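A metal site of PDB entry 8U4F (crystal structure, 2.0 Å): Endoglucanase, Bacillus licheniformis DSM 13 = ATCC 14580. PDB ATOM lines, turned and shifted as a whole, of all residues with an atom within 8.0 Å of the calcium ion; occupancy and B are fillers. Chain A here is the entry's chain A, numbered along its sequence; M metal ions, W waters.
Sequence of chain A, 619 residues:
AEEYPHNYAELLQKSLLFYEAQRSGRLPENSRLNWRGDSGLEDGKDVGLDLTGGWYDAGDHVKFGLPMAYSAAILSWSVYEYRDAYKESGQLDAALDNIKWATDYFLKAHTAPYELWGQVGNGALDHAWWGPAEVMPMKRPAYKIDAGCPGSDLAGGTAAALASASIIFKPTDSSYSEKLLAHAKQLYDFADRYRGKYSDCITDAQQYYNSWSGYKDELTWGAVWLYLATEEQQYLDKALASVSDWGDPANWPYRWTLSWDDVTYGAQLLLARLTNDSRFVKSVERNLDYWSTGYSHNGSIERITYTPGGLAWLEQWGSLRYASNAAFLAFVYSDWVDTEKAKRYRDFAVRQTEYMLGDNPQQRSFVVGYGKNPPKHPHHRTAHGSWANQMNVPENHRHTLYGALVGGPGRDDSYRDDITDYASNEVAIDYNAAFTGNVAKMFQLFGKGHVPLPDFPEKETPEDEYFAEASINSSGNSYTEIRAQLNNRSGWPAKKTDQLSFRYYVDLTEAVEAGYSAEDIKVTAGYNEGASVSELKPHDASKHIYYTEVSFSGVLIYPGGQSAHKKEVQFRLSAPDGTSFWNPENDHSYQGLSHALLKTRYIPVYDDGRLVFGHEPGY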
ATOM      1  N   THR A 480      33.346  -2.412 -27.194  1.00  0.00           N
ATOM      2  CA  THR A 480      33.899  -2.119 -28.498  1.00  0.00           C
ATOM      3  C   THR A 480      35.398  -1.946 -28.303  1.00  0.00           C
ATOM      4  O   THR A 480      35.823  -1.199 -27.414  1.00  0.00           O
ATOM      5  CB  THR A 480      33.311  -0.848 -29.126  1.00  0.00           C
ATOM      6  OG1 THR A 480      31.920  -1.044 -29.396  1.00  0.00           O
ATOM      7  CG2 THR A 480      34.006  -0.527 -30.439  1.00  0.00           C
ATOM      8  N   TYR A 505      34.118   9.269 -29.378  1.00  0.00           N
ATOM      9  CA  TYR A 505      32.832   9.615 -28.797  1.00  0.00           C
ATOM     10  C   TYR A 505      31.851   8.458 -28.908  1.00  0.00           C
ATOM     11  O   TYR A 505      31.760   7.800 -29.956  1.00  0.00           O
ATOM     12  CB  TYR A 505      32.248  10.851 -29.478  1.00  0.00           C
ATOM     13  CG  TYR A 505      33.027  12.129 -29.234  1.00  0.00           C
ATOM     14  CD1 TYR A 505      34.126  12.469 -30.022  1.00  0.00           C
ATOM     15  CD2 TYR A 505      32.657  13.009 -28.228  1.00  0.00           C
ATOM     16  CE1 TYR A 505      34.843  13.655 -29.805  1.00  0.00           C
ATOM     17  CE2 TYR A 505      33.352  14.179 -27.999  1.00  0.00           C
ATOM     18  CZ  TYR A 505      34.448  14.505 -28.785  1.00  0.00           C
ATOM     19  OH  TYR A 505      35.142  15.676 -28.556  1.00  0.00           O
ATOM     20  N   VAL A 506      31.106   8.226 -27.831  1.00  0.00           N
ATOM     21  CA  VAL A 506      30.056   7.216 -27.774  1.00  0.00           C
ATOM     22  C   VAL A 506      28.751   7.886 -27.322  1.00  0.00           C
ATOM     23  O   VAL A 506      28.747   8.993 -26.777  1.00  0.00           O
ATOM     24  CB  VAL A 506      30.399   6.056 -26.822  1.00  0.00           C
ATOM     25  CG1 VAL A 506      31.700   5.391 -27.226  1.00  0.00           C
ATOM     26  CG2 VAL A 506      30.466   6.550 -25.366  1.00  0.00           C
ATOM     27  N   ASP A 507      27.654   7.182 -27.572  1.00  0.00           N
ATOM     28  CA  ASP A 507      26.332   7.560 -27.108  1.00  0.00           C
ATOM     29  C   ASP A 507      25.905   6.525 -26.069  1.00  0.00           C
ATOM     30  O   ASP A 507      25.896   5.331 -26.350  1.00  0.00           O
ATOM     31  CB  ASP A 507      25.344   7.598 -28.275  1.00  0.00           C
ATOM     32  CG  ASP A 507      23.937   8.081 -27.883  1.00  0.00           C
ATOM     33  OD1 ASP A 507      23.485   7.838 -26.734  1.00  0.00           O
ATOM     34  OD2 ASP A 507      23.279   8.713 -28.727  1.00  0.00           O
ATOM     35  N   LEU A 508      25.564   6.991 -24.861  1.00  0.00           N
ATOM     36  CA  LEU A 508      25.217   6.074 -23.789  1.00  0.00           C
ATOM     37  C   LEU A 508      23.717   5.998 -23.521  1.00  0.00           C
ATOM     38  O   LEU A 508      23.316   5.480 -22.482  1.00  0.00           O
ATOM     39  CB  LEU A 508      25.963   6.453 -22.510  1.00  0.00           C
ATOM     40  CG  LEU A 508      27.474   6.226 -22.516  1.00  0.00           C
ATOM     41  CD1 LEU A 508      27.942   6.054 -21.079  1.00  0.00           C
ATOM     42  CD2 LEU A 508      27.851   5.012 -23.360  1.00  0.00           C
ATOM     43  N   THR A 509      22.896   6.489 -24.447  1.00  0.00           N
ATOM     44  CA  THR A 509      21.451   6.416 -24.254  1.00  0.00           C
ATOM     45  C   THR A 509      21.003   4.997 -23.923  1.00  0.00           C
ATOM     46  O   THR A 509      20.267   4.780 -22.962  1.00  0.00           O
ATOM     47  CB  THR A 509      20.719   6.931 -25.498  1.00  0.00           C
ATOM     48  OG1 THR A 509      21.030   8.319 -25.696  1.00  0.00           O
ATOM     49  CG2 THR A 509      19.213   6.772 -25.345  1.00  0.00           C
ATOM     50  N   GLU A 510      21.490   4.015 -24.686  1.00  0.00           N
ATOM     51  CA  GLU A 510      21.077   2.636 -24.455  1.00  0.00           C
ATOM     52  C   GLU A 510      21.537   2.147 -23.086  1.00  0.00           C
ATOM     53  O   GLU A 510      20.884   1.282 -22.490  1.00  0.00           O
ATOM     54  CB  GLU A 510      21.602   1.714 -25.561  1.00  0.00           C
ATOM     55  CG  GLU A 510      23.068   1.319 -25.452  1.00  0.00           C
ATOM     56  CD  GLU A 510      24.006   2.241 -26.198  1.00  0.00           C
ATOM     57  OE1 GLU A 510      23.552   3.276 -26.732  1.00  0.00           O
ATOM     58  OE2 GLU A 510      25.208   1.928 -26.250  1.00  0.00           O
ATOM     59  N   ALA A 511      22.641   2.688 -22.562  1.00  0.00           N
ATOM     60  CA  ALA A 511      23.092   2.322 -21.219  1.00  0.00           C
ATOM     61  C   ALA A 511      22.170   2.895 -20.147  1.00  0.00           C
ATOM     62  O   ALA A 511      21.788   2.190 -19.200  1.00  0.00           O
ATOM     63  CB  ALA A 511      24.534   2.814 -20.998  1.00  0.00           C
ATOM     64  N   HIS A 544      23.539  12.175 -23.349  1.00  0.00           N
ATOM     65  CA  HIS A 544      24.317  11.019 -22.926  1.00  0.00           C
ATOM     66  C   HIS A 544      25.498  10.756 -23.842  1.00  0.00           C
ATOM     67  O   HIS A 544      25.863   9.609 -24.105  1.00  0.00           O
ATOM     68  CB  HIS A 544      23.424   9.785 -22.813  1.00  0.00           C
ATOM     69  CG  HIS A 544      22.187  10.014 -22.000  1.00  0.00           C
ATOM     70  ND1 HIS A 544      22.231  10.255 -20.641  1.00  0.00           N
ATOM     71  CD2 HIS A 544      20.884  10.075 -22.348  1.00  0.00           C
ATOM     72  CE1 HIS A 544      21.011  10.430 -20.184  1.00  0.00           C
ATOM     73  NE2 HIS A 544      20.171  10.329 -21.205  1.00  0.00           N
ATOM     74  N   ILE A 545      26.114  11.832 -24.353  1.00  0.00           N
ATOM     75  CA  ILE A 545      27.273  11.724 -25.221  1.00  0.00           C
ATOM     76  C   ILE A 545      28.522  11.869 -24.366  1.00  0.00           C
ATOM     77  O   ILE A 545      28.642  12.821 -23.584  1.00  0.00           O
ATOM     78  CB  ILE A 545      27.242  12.765 -26.347  1.00  0.00           C
ATOM     79  CG1 ILE A 545      25.883  12.758 -27.054  1.00  0.00           C
ATOM     80  CG2 ILE A 545      28.371  12.506 -27.333  1.00  0.00           C
ATOM     81  CD1 ILE A 545      25.455  11.406 -27.610  1.00  0.00           C
ATOM     82  N   PHE A 581      23.559  -4.511 -23.079  1.00  0.00           N
ATOM     83  CA  PHE A 581      22.923  -3.323 -23.619  1.00  0.00           C
ATOM     84  C   PHE A 581      23.799  -2.557 -24.599  1.00  0.00           C
ATOM     85  O   PHE A 581      23.263  -1.793 -25.404  1.00  0.00           O
ATOM     86  CB  PHE A 581      22.478  -2.399 -22.475  1.00  0.00           C
ATOM     87  CG  PHE A 581      23.608  -1.944 -21.601  1.00  0.00           C
ATOM     88  CD1 PHE A 581      24.483  -0.948 -22.023  1.00  0.00           C
ATOM     89  CD2 PHE A 581      23.804  -2.514 -20.360  1.00  0.00           C
ATOM     90  CE1 PHE A 581      25.530  -0.534 -21.221  1.00  0.00           C
ATOM     91  CE2 PHE A 581      24.851  -2.092 -19.547  1.00  0.00           C
ATOM     92  CZ  PHE A 581      25.702  -1.099 -19.974  1.00  0.00           C
ATOM     93  N   TRP A 582      25.128  -2.747 -24.552  1.00  0.00           N
ATOM     94  CA  TRP A 582      26.058  -1.897 -25.299  1.00  0.00           C
ATOM     95  C   TRP A 582      25.747  -1.879 -26.790  1.00  0.00           C
ATOM     96  O   TRP A 582      25.603  -2.934 -27.417  1.00  0.00           O
ATOM     97  CB  TRP A 582      27.489  -2.380 -25.063  1.00  0.00           C
ATOM     98  CG  TRP A 582      28.549  -1.584 -25.795  1.00  0.00           C
ATOM     99  CD1 TRP A 582      29.126  -1.896 -26.995  1.00  0.00           C
ATOM    100  CD2 TRP A 582      29.159  -0.354 -25.360  1.00  0.00           C
ATOM    101  NE1 TRP A 582      30.047  -0.931 -27.344  1.00  0.00           N
ATOM    102  CE2 TRP A 582      30.091   0.028 -26.363  1.00  0.00           C
ATOM    103  CE3 TRP A 582      29.013   0.463 -24.232  1.00  0.00           C
ATOM    104  CZ2 TRP A 582      30.864   1.176 -26.261  1.00  0.00           C
ATOM    105  CZ3 TRP A 582      29.776   1.613 -24.140  1.00  0.00           C
ATOM    106  CH2 TRP A 582      30.698   1.966 -25.156  1.00  0.00           C
ATOM    107  N   ASN A 583      25.653  -0.683 -27.362  1.00  0.00           N
ATOM    108  CA  ASN A 583      25.316  -0.492 -28.775  1.00  0.00           C
ATOM    109  C   ASN A 583      26.251   0.511 -29.440  1.00  0.00           C
ATOM    110  O   ASN A 583      26.076   1.738 -29.280  1.00  0.00           O
ATOM    111  CB  ASN A 583      23.869  -0.056 -28.933  1.00  0.00           C
ATOM    112  CG  ASN A 583      23.460   0.080 -30.391  1.00  0.00           C
ATOM    113  OD1 ASN A 583      24.162  -0.379 -31.289  1.00  0.00           O
ATOM    114  ND2 ASN A 583      22.331   0.748 -30.626  1.00  0.00           N
ATOM    115  N   PRO A 584      27.222   0.049 -30.237  1.00  0.00           N
ATOM    116  CA  PRO A 584      28.143   0.991 -30.884  1.00  0.00           C
ATOM    117  C   PRO A 584      27.526   1.736 -32.055  1.00  0.00           C
ATOM    118  O   PRO A 584      28.053   2.776 -32.457  1.00  0.00           O
ATOM    119  CB  PRO A 584      29.272   0.079 -31.362  1.00  0.00           C
ATOM    120  CG  PRO A 584      28.541  -1.192 -31.727  1.00  0.00           C
ATOM    121  CD  PRO A 584      27.419  -1.330 -30.708  1.00  0.00           C
ATOM    122  N   GLU A 585      26.421   1.234 -32.617  1.00  0.00           N
ATOM    123  CA  GLU A 585      25.912   1.767 -33.867  1.00  0.00           C
ATOM    124  C   GLU A 585      25.428   3.207 -33.741  1.00  0.00           C
ATOM    125  O   GLU A 585      25.405   3.925 -34.747  1.00  0.00           O
ATOM    126  CB  GLU A 585      24.776   0.882 -34.404  1.00  0.00           C
ATOM    127  CG  GLU A 585      25.177  -0.570 -34.675  1.00  0.00           C
ATOM    128  CD  GLU A 585      26.298  -0.718 -35.723  1.00  0.00           C
ATOM    129  OE1 GLU A 585      26.374   0.118 -36.653  1.00  0.00           O
ATOM    130  OE2 GLU A 585      27.102  -1.678 -35.609  1.00  0.00           O
ATOM    131  N   ASN A 586      25.070   3.668 -32.546  1.00  0.00           N
ATOM    132  CA  ASN A 586      24.732   5.070 -32.356  1.00  0.00           C
ATOM    133  C   ASN A 586      25.903   5.897 -31.814  1.00  0.00           C
ATOM    134  O   ASN A 586      25.714   7.061 -31.450  1.00  0.00           O
ATOM    135  CB  ASN A 586      23.500   5.219 -31.452  1.00  0.00           C
ATOM    136  CG  ASN A 586      23.707   4.701 -30.031  1.00  0.00           C
ATOM    137  OD1 ASN A 586      24.812   4.361 -29.612  1.00  0.00           O
ATOM    138  ND2 ASN A 586      22.625   4.645 -29.266  1.00  0.00           N
ATOM    139  N   ASP A 587      27.111   5.331 -31.778  1.00  0.00           N
ATOM    140  CA  ASP A 587      28.275   6.047 -31.278  1.00  0.00           C
ATOM    141  C   ASP A 587      28.900   6.881 -32.391  1.00  0.00           C
ATOM    142  O   ASP A 587      29.187   6.380 -33.475  1.00  0.00           O
ATOM    143  CB  ASP A 587      29.316   5.060 -30.712  1.00  0.00           C
ATOM    144  CG  ASP A 587      28.829   4.382 -29.421  1.00  0.00           C
ATOM    145  OD1 ASP A 587      27.789   4.789 -28.879  1.00  0.00           O
ATOM    146  OD2 ASP A 587      29.504   3.448 -28.945  1.00  0.00           O
ATOM    147  N   HIS A 588      29.104   8.174 -32.096  1.00  0.00           N
ATOM    148  CA  HIS A 588      29.617   9.130 -33.083  1.00  0.00           C
ATOM    149  C   HIS A 588      30.884   8.633 -33.771  1.00  0.00           C
ATOM    150  O   HIS A 588      30.977   8.664 -35.012  1.00  0.00           O
ATOM    151  CB  HIS A 588      29.871  10.474 -32.390  1.00  0.00           C
ATOM    152  CG  HIS A 588      30.540  11.497 -33.266  1.00  0.00           C
ATOM    153  ND1 HIS A 588      29.843  12.270 -34.166  1.00  0.00           N
ATOM    154  CD2 HIS A 588      31.836  11.879 -33.361  1.00  0.00           C
ATOM    155  CE1 HIS A 588      30.683  13.079 -34.791  1.00  0.00           C
ATOM    156  NE2 HIS A 588      31.895  12.860 -34.317  1.00  0.00           N
ATOM    157  N   TYR A 590      32.179   5.665 -33.995  1.00  0.00           N
ATOM    158  CA  TYR A 590      32.086   4.341 -34.588  1.00  0.00           C
ATOM    159  C   TYR A 590      31.634   4.386 -36.030  1.00  0.00           C
ATOM    160  O   TYR A 590      31.802   3.402 -36.750  1.00  0.00           O
ATOM    161  CB  TYR A 590      31.094   3.511 -33.765  1.00  0.00           C
ATOM    162  CG  TYR A 590      31.076   2.018 -34.012  1.00  0.00           C
ATOM    163  CD1 TYR A 590      32.086   1.204 -33.517  1.00  0.00           C
ATOM    164  CD2 TYR A 590      30.020   1.416 -34.678  1.00  0.00           C
ATOM    165  CE1 TYR A 590      32.052  -0.156 -33.694  1.00  0.00           C
ATOM    166  CE2 TYR A 590      29.979   0.041 -34.870  1.00  0.00           C
ATOM    167  CZ  TYR A 590      30.996  -0.736 -34.367  1.00  0.00           C
ATOM    168  OH  TYR A 590      30.968  -2.098 -34.551  1.00  0.00           O
HETATM  169 CA    CA M   1      26.019   3.501 -27.792  1.00  0.00          CA
HETATM  170  O   HOH W   1      27.973   2.723 -27.020  1.00  0.00           O
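Five residues have an atom within 4 Å of the calcium ion: Asp 507, Glu 510, Asn 583, Asn 586 and Asp 587.
The nearest printed residue that does not touch the calcium ion is Pro 584 (4.4 Å).
The side-chain amide oxygen (OD1) of Asn 583 sits at hydrogen-bond distance from the backbone NH (N) of Glu 585 (3.1 Å).
The side-chain carboxylate (OD1) of Asp 507 sits at hydrogen-bond distance from the side-chain hydroxyl (OG1) of Thr 509 (2.7 Å).
The calcium ion is bound by water W1 (2.2 Å), O of Asn 583 (2.3 Å), O of Asp 507 (2.3 Å), OD1 of Asn 586 (2.3 Å), OE2 of Glu 510 (2.3 Å), OD1 of Asp 587 (2.4 Å) and OE1 of Glu 510 (2.7 Å).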
